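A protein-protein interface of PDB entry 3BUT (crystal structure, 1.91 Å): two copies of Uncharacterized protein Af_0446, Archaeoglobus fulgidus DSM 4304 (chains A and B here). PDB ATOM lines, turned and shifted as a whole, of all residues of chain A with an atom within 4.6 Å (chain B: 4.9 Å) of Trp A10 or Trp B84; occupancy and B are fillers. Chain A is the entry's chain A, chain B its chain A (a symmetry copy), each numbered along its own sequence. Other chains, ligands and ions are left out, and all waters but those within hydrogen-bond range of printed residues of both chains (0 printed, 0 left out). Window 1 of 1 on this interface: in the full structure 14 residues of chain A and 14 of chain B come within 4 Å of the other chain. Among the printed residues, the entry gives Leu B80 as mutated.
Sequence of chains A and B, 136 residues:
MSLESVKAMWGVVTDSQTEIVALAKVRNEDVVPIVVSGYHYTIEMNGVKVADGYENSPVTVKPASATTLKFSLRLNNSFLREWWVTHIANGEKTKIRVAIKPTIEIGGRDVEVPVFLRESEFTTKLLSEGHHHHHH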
ATOM      1  N   MET A   9     -14.312  -5.896 -31.178  1.00  0.00           N
ATOM      2  CA  MET A   9     -14.982  -5.909 -29.884  1.00  0.00           C
ATOM      3  C   MET A   9     -16.455  -5.601 -30.092  1.00  0.00           C
ATOM      4  O   MET A   9     -16.839  -5.092 -31.144  1.00  0.00           O
ATOM      5  CB  MET A   9     -14.355  -4.894 -28.927  1.00  0.00           C
ATOM      6  CG  MET A   9     -13.943  -3.601 -29.578  1.00  0.00           C
ATOM      7  SD  MET A   9     -13.308  -2.313 -28.292  1.00  0.00           S
ATOM      8  CE  MET A   9     -12.412  -3.508 -27.030  1.00  0.00           C
ATOM      9  N   TRP A  10     -17.279  -5.930 -29.100  1.00  0.00           N
ATOM     10  CA  TRP A  10     -18.695  -5.588 -29.157  1.00  0.00           C
ATOM     11  C   TRP A  10     -18.863  -4.101 -28.877  1.00  0.00           C
ATOM     12  O   TRP A  10     -18.112  -3.520 -28.096  1.00  0.00           O
ATOM     13  CB  TRP A  10     -19.517  -6.421 -28.162  1.00  0.00           C
ATOM     14  CG  TRP A  10     -19.515  -7.897 -28.458  1.00  0.00           C
ATOM     15  CD1 TRP A  10     -18.847  -8.866 -27.770  1.00  0.00           C
ATOM     16  CD2 TRP A  10     -20.201  -8.563 -29.522  1.00  0.00           C
ATOM     17  NE1 TRP A  10     -19.080 -10.093 -28.332  1.00  0.00           N
ATOM     18  CE2 TRP A  10     -19.905  -9.937 -29.413  1.00  0.00           C
ATOM     19  CE3 TRP A  10     -21.037  -8.131 -30.560  1.00  0.00           C
ATOM     20  CZ2 TRP A  10     -20.413 -10.883 -30.300  1.00  0.00           C
ATOM     21  CZ3 TRP A  10     -21.544  -9.070 -31.437  1.00  0.00           C
ATOM     22  CH2 TRP A  10     -21.229 -10.432 -31.302  1.00  0.00           C
ATOM     23  N   GLY A  11     -19.843  -3.492 -29.533  1.00  0.00           N
ATOM     24  CA  GLY A  11     -20.181  -2.095 -29.286  1.00  0.00           C
ATOM     25  C   GLY A  11     -21.492  -1.998 -28.547  1.00  0.00           C
ATOM     26  O   GLY A  11     -21.860  -2.913 -27.807  1.00  0.00           O
ATOM     27  N   VAL A  13     -25.004  -2.539 -27.892  1.00  0.00           N
ATOM     28  CA  VAL A  13     -25.973  -3.520 -28.339  1.00  0.00           C
ATOM     29  C   VAL A  13     -27.300  -3.276 -27.641  1.00  0.00           C
ATOM     30  O   VAL A  13     -27.369  -3.196 -26.412  1.00  0.00           O
ATOM     31  CB  VAL A  13     -25.456  -4.950 -28.119  1.00  0.00           C
ATOM     32  CG1 VAL A  13     -26.533  -5.990 -28.430  1.00  0.00           C
ATOM     33  CG2 VAL A  13     -24.219  -5.186 -28.983  1.00  0.00           C
ATOM     34  N   THR A  18     -27.425  -4.508 -33.236  1.00  0.00           N
ATOM     35  CA  THR A  18     -26.187  -5.040 -32.660  1.00  0.00           C
ATOM     36  C   THR A  18     -24.999  -4.397 -33.370  1.00  0.00           C
ATOM     37  O   THR A  18     -24.943  -4.391 -34.597  1.00  0.00           O
ATOM     38  CB  THR A  18     -26.117  -6.587 -32.820  1.00  0.00           C
ATOM     39  OG1 THR A  18     -27.268  -7.192 -32.217  1.00  0.00           O
ATOM     40  CG2 THR A  18     -24.847  -7.167 -32.193  1.00  0.00           C
ATOM     41  N   GLU A  19     -24.052  -3.863 -32.600  1.00  0.00           N
ATOM     42  CA  GLU A  19     -22.857  -3.235 -33.165  1.00  0.00           C
ATOM     43  C   GLU A  19     -21.602  -4.048 -32.885  1.00  0.00           C
ATOM     44  O   GLU A  19     -21.394  -4.534 -31.780  1.00  0.00           O
ATOM     45  CB  GLU A  19     -22.692  -1.810 -32.622  1.00  0.00           C
ATOM     46  CG  GLU A  19     -21.516  -1.020 -33.213  1.00  0.00           C
ATOM     47  CD  GLU A  19     -21.228   0.260 -32.450  1.00  0.00           C
ATOM     48  OE1 GLU A  19     -21.900   0.520 -31.432  1.00  0.00           O
ATOM     49  OE2 GLU A  19     -20.322   1.009 -32.865  1.00  0.00           O
ATOM     50  N   ILE A  20     -20.786  -4.204 -33.917  1.00  0.00           N
ATOM     51  CA  ILE A  20     -19.451  -4.745 -33.775  1.00  0.00           C
ATOM     52  C   ILE A  20     -18.508  -3.603 -34.126  1.00  0.00           C
ATOM     53  O   ILE A  20     -18.746  -2.884 -35.093  1.00  0.00           O
ATOM     54  CB  ILE A  20     -19.231  -5.964 -34.698  1.00  0.00           C
ATOM     55  CG1 ILE A  20     -20.237  -7.071 -34.355  1.00  0.00           C
ATOM     56  CG2 ILE A  20     -17.802  -6.494 -34.571  1.00  0.00           C
ATOM     57  CD1 ILE A  20     -20.362  -8.169 -35.409  1.00  0.00           C
ATOM     58  N   VAL A  21     -17.465  -3.417 -33.321  1.00  0.00           N
ATOM     59  CA  VAL A  21     -16.492  -2.362 -33.555  1.00  0.00           C
ATOM     60  C   VAL A  21     -15.153  -2.986 -33.910  1.00  0.00           C
ATOM     61  O   VAL A  21     -14.603  -3.765 -33.134  1.00  0.00           O
ATOM     62  CB  VAL A  21     -16.322  -1.435 -32.319  1.00  0.00           C
ATOM     63  CG1 VAL A  21     -15.395  -0.265 -32.641  1.00  0.00           C
ATOM     64  CG2 VAL A  21     -17.661  -0.913 -31.840  1.00  0.00           C
ATOM     65  N   LEU B  80     -36.758 -13.254 -27.725  1.00  0.00           N
ATOM     66  CA  LEU B  80     -35.414 -13.780 -27.971  1.00  0.00           C
ATOM     67  C   LEU B  80     -34.417 -12.688 -28.307  1.00  0.00           C
ATOM     68  O   LEU B  80     -33.227 -12.851 -28.057  1.00  0.00           O
ATOM     69  CB  LEU B  80     -35.415 -14.824 -29.084  1.00  0.00           C
ATOM     70  CG  LEU B  80     -35.342 -16.296 -28.693  1.00  0.00           C
ATOM     71  CD1 LEU B  80     -35.788 -17.147 -29.864  1.00  0.00           C
ATOM     72  CD2 LEU B  80     -33.927 -16.664 -28.268  1.00  0.00           C
ATOM     73  N   ARG B  81     -34.904 -11.577 -28.861  1.00  0.00           N
ATOM     74  CA  ARG B  81     -34.043 -10.441 -29.214  1.00  0.00           C
ATOM     75  C   ARG B  81     -33.573  -9.632 -28.001  1.00  0.00           C
ATOM     76  O   ARG B  81     -32.630  -8.837 -28.109  1.00  0.00           O
ATOM     77  CB  ARG B  81     -34.730  -9.506 -30.213  1.00  0.00           C
ATOM     78  CG  ARG B  81     -34.852 -10.050 -31.630  1.00  0.00           C
ATOM     79  CD  ARG B  81     -35.528  -9.045 -32.571  1.00  0.00           C
ATOM     80  NE  ARG B  81     -36.881  -8.669 -32.149  1.00  0.00           N
ATOM     81  CZ  ARG B  81     -37.219  -7.483 -31.641  1.00  0.00           C
ATOM     82  NH1 ARG B  81     -36.308  -6.531 -31.481  1.00  0.00           N
ATOM     83  NH2 ARG B  81     -38.475  -7.249 -31.289  1.00  0.00           N
ATOM     84  N   GLU B  82     -34.234  -9.805 -26.861  1.00  0.00           N
ATOM     85  CA  GLU B  82     -33.774  -9.135 -25.650  1.00  0.00           C
ATOM     86  C   GLU B  82     -32.911 -10.052 -24.793  1.00  0.00           C
ATOM     87  O   GLU B  82     -32.336  -9.619 -23.800  1.00  0.00           O
ATOM     88  CB  GLU B  82     -34.923  -8.490 -24.863  1.00  0.00           C
ATOM     89  CG  GLU B  82     -36.054  -9.411 -24.456  1.00  0.00           C
ATOM     90  CD  GLU B  82     -37.112  -8.697 -23.635  1.00  0.00           C
ATOM     91  OE1 GLU B  82     -37.516  -7.576 -24.023  1.00  0.00           O
ATOM     92  OE2 GLU B  82     -37.544  -9.260 -22.606  1.00  0.00           O
ATOM     93  N   TRP B  83     -32.807 -11.314 -25.202  1.00  0.00           N
ATOM     94  CA  TRP B  83     -31.871 -12.246 -24.580  1.00  0.00           C
ATOM     95  C   TRP B  83     -30.465 -11.928 -25.061  1.00  0.00           C
ATOM     96  O   TRP B  83     -29.514 -11.966 -24.285  1.00  0.00           O
ATOM     97  CB  TRP B  83     -32.222 -13.711 -24.900  1.00  0.00           C
ATOM     98  CG  TRP B  83     -31.001 -14.604 -24.948  1.00  0.00           C
ATOM     99  CD1 TRP B  83     -30.297 -15.085 -23.885  1.00  0.00           C
ATOM    100  CD2 TRP B  83     -30.315 -15.067 -26.122  1.00  0.00           C
ATOM    101  NE1 TRP B  83     -29.233 -15.832 -24.319  1.00  0.00           N
ATOM    102  CE2 TRP B  83     -29.217 -15.836 -25.686  1.00  0.00           C
ATOM    103  CE3 TRP B  83     -30.527 -14.908 -27.499  1.00  0.00           C
ATOM    104  CZ2 TRP B  83     -28.331 -16.448 -26.572  1.00  0.00           C
ATOM    105  CZ3 TRP B  83     -29.650 -15.520 -28.380  1.00  0.00           C
ATOM    106  CH2 TRP B  83     -28.566 -16.285 -27.912  1.00  0.00           C
ATOM    107  N   TRP B  84     -30.349 -11.616 -26.348  1.00  0.00           N
ATOM    108  CA  TRP B  84     -29.060 -11.391 -26.984  1.00  0.00           C
ATOM    109  C   TRP B  84     -28.167 -10.404 -26.233  1.00  0.00           C
ATOM    110  O   TRP B  84     -26.965 -10.639 -26.087  1.00  0.00           O
ATOM    111  CB  TRP B  84     -29.235 -10.983 -28.452  1.00  0.00           C
ATOM    112  CG  TRP B  84     -27.925 -10.726 -29.123  1.00  0.00           C
ATOM    113  CD1 TRP B  84     -27.458  -9.527 -29.563  1.00  0.00           C
ATOM    114  CD2 TRP B  84     -26.886 -11.685 -29.383  1.00  0.00           C
ATOM    115  NE1 TRP B  84     -26.200  -9.677 -30.100  1.00  0.00           N
ATOM    116  CE2 TRP B  84     -25.827 -10.992 -30.000  1.00  0.00           C
ATOM    117  CE3 TRP B  84     -26.756 -13.065 -29.165  1.00  0.00           C
ATOM    118  CZ2 TRP B  84     -24.651 -11.628 -30.403  1.00  0.00           C
ATOM    119  CZ3 TRP B  84     -25.587 -13.696 -29.563  1.00  0.00           C
ATOM    120  CH2 TRP B  84     -24.551 -12.977 -30.173  1.00  0.00           C
ATOM    121  N   VAL B  85     -28.771  -9.325 -25.735  1.00  0.00           N
ATOM    122  CA  VAL B  85     -28.098  -8.351 -24.873  1.00  0.00           C
ATOM    123  C   VAL B  85     -27.387  -9.034 -23.702  1.00  0.00           C
ATOM    124  O   VAL B  85     -26.205  -8.785 -23.459  1.00  0.00           O
ATOM    125  CB  VAL B  85     -29.108  -7.314 -24.305  1.00  0.00           C
ATOM    126  CG1 VAL B  85     -28.389  -6.221 -23.513  1.00  0.00           C
ATOM    127  CG2 VAL B  85     -29.950  -6.701 -25.422  1.00  0.00           C
ATOM    128  N   THR B  86     -28.118  -9.909 -23.013  1.00  0.00           N
ATOM    129  CA  THR B  86     -27.644 -10.586 -21.804  1.00  0.00           C
ATOM    130  C   THR B  86     -26.559 -11.611 -22.103  1.00  0.00           C
ATOM    131  O   THR B  86     -25.667 -11.833 -21.280  1.00  0.00           O
ATOM    132  CB  THR B  86     -28.799 -11.289 -21.040  1.00  0.00           C
ATOM    133  OG1 THR B  86     -29.249 -12.436 -21.770  1.00  0.00           O
ATOM    134  CG2 THR B  86     -29.968 -10.362 -20.843  1.00  0.00           C
ATOM    135  N   HIS B  87     -26.655 -12.237 -23.274  1.00  0.00           N
ATOM    136  CA  HIS B  87     -25.697 -13.249 -23.696  1.00  0.00           C
ATOM    137  C   HIS B  87     -24.307 -12.650 -23.797  1.00  0.00           C
ATOM    138  O   HIS B  87     -23.396 -13.105 -23.121  1.00  0.00           O
ATOM    139  CB  HIS B  87     -26.103 -13.895 -25.024  1.00  0.00           C
ATOM    140  CG  HIS B  87     -25.104 -14.883 -25.541  1.00  0.00           C
ATOM    141  ND1 HIS B  87     -24.953 -16.142 -24.999  1.00  0.00           N
ATOM    142  CD2 HIS B  87     -24.200 -14.797 -26.544  1.00  0.00           C
ATOM    143  CE1 HIS B  87     -24.007 -16.791 -25.652  1.00  0.00           C
ATOM    144  NE2 HIS B  87     -23.533 -15.996 -26.595  1.00  0.00           N
ATOM    145  N   ILE B  88     -24.158 -11.611 -24.611  1.00  0.00           N
ATOM    146  CA  ILE B  88     -22.863 -10.949 -24.756  1.00  0.00           C
ATOM    147  C   ILE B  88     -22.430 -10.222 -23.482  1.00  0.00           C
ATOM    148  O   ILE B  88     -21.246 -10.227 -23.158  1.00  0.00           O
ATOM    149  CB  ILE B  88     -22.795 -10.014 -25.977  1.00  0.00           C
ATOM    150  CG1 ILE B  88     -23.932  -9.002 -25.952  1.00  0.00           C
ATOM    151  CG2 ILE B  88     -22.813 -10.822 -27.282  1.00  0.00           C
ATOM    152  CD1 ILE B  88     -23.574  -7.758 -26.630  1.00  0.00           C
ATOM    153  N   GLU B  92     -20.503 -13.709 -23.545  1.00  0.00           N
ATOM    154  CA  GLU B  92     -21.088 -14.716 -24.440  1.00  0.00           C
ATOM    155  C   GLU B  92     -21.370 -16.053 -23.749  1.00  0.00           C
ATOM    156  O   GLU B  92     -21.019 -17.111 -24.258  1.00  0.00           O
ATOM    157  CB  GLU B  92     -20.255 -14.890 -25.711  1.00  0.00           C
ATOM    158  CG  GLU B  92     -20.251 -13.684 -26.631  1.00  0.00           C
ATOM    159  CD  GLU B  92     -19.286 -13.847 -27.774  1.00  0.00           C
ATOM    160  OE1 GLU B  92     -19.568 -14.662 -28.678  1.00  0.00           O
ATOM    161  OE2 GLU B  92     -18.246 -13.158 -27.766  1.00  0.00           O
ATOM    162  N   LEU B 126     -17.596 -15.557 -30.921  1.00  0.00           N
ATOM    163  CA  LEU B 126     -17.856 -15.067 -32.275  1.00  0.00           C
ATOM    164  C   LEU B 126     -16.782 -14.144 -32.840  1.00  0.00           C
ATOM    165  O   LEU B 126     -16.506 -14.176 -34.042  1.00  0.00           O
ATOM    166  CB  LEU B 126     -19.222 -14.381 -32.339  1.00  0.00           C
ATOM    167  CG  LEU B 126     -20.434 -15.235 -31.967  1.00  0.00           C
ATOM    168  CD1 LEU B 126     -21.680 -14.380 -31.950  1.00  0.00           C
ATOM    169  CD2 LEU B 126     -20.601 -16.402 -32.919  1.00  0.00           C
ATOM    170  N   LEU B 127     -16.183 -13.327 -31.979  1.00  0.00           N
ATOM    171  CA  LEU B 127     -15.182 -12.362 -32.415  1.00  0.00           C
ATOM    172  C   LEU B 127     -13.768 -12.876 -32.166  1.00  0.00           C
ATOM    173  O   LEU B 127     -13.210 -13.604 -32.986  1.00  0.00           O
ATOM    174  CB  LEU B 127     -15.383 -11.012 -31.717  1.00  0.00           C
ATOM    175  CG  LEU B 127     -16.787 -10.409 -31.608  1.00  0.00           C
ATOM    176  CD1 LEU B 127     -16.708  -9.123 -30.836  1.00  0.00           C
ATOM    177  CD2 LEU B 127     -17.420 -10.163 -32.965  1.00  0.00           C
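No position is printed for both chains. Of the 8 pairs that touch across the chains among the printed residues, none has its exchanged pair printed and touching as well.
Of the printed residues of chain B, Met A9 touches Leu B127. Of the printed residues of chain B, Thr A18 touches Trp B84. Glu A19 touches none of the printed residues of chain B. Glu B82 touches none of the printed residues of chain A. Trp B84 touches just these residues of chain A: Trp A10, Val A13 and Thr A18. Printed residues of chain A within 4 Å of Ile B88: Trp A10 and Val A13. The nearest printed residue of chain B that does not touch Met A9 is Glu B92 (8.1 Å).
NE1 of Trp B84 lies within hydrogen-bond range of OG1 of Thr A18 (3.4 Å). NE1 of Trp A10 sits at hydrogen-bond distance from OE2 of Glu B92, 3.2 Å away.
Of the 8 printed residues of chain A, 4 touch a printed residue of chain B. Hydrophobic or aromatic side chains of chain A within 4 Å of the printed part of chain B: Trp A10 and Val A13. Of the 12 printed residues of chain B, 4 touch a printed residue of chain A. Hydrophobic or aromatic side chains of chain B within 4 Å of the printed part of chain A: Trp B84, Ile B88 and Leu B127. Among the printed residues, no Asp or Glu carboxylate lies within 4 Å of a Lys or Arg side-chain nitrogen of the other chain.
OE1 of Glu B92 is in hydrogen-bond range of N of Leu B126. The backbone carbonyl oxygen of His B87 lies within hydrogen-bond range of the backbone NH of Glu B92 (3.0 Å). The backbone NH of Val A21 lies within hydrogen-bond range of the backbone carbonyl oxygen of Met A9.
C of Met A9 touches CD1 of Leu B127, at 3.6 Å. CZ2 of Trp B84 touches CH2 of Trp A10 (3.7 Å). Ile B88 touches Trp A10 (CG2 to CE2, 3.7 Å). Trp A10 touches Leu B127. Val A13 touches Trp B84 (CG1 to CD1, 3.8 Å). CG2 of Val A13 touches CD1 of Ile B88 (3.5 Å).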
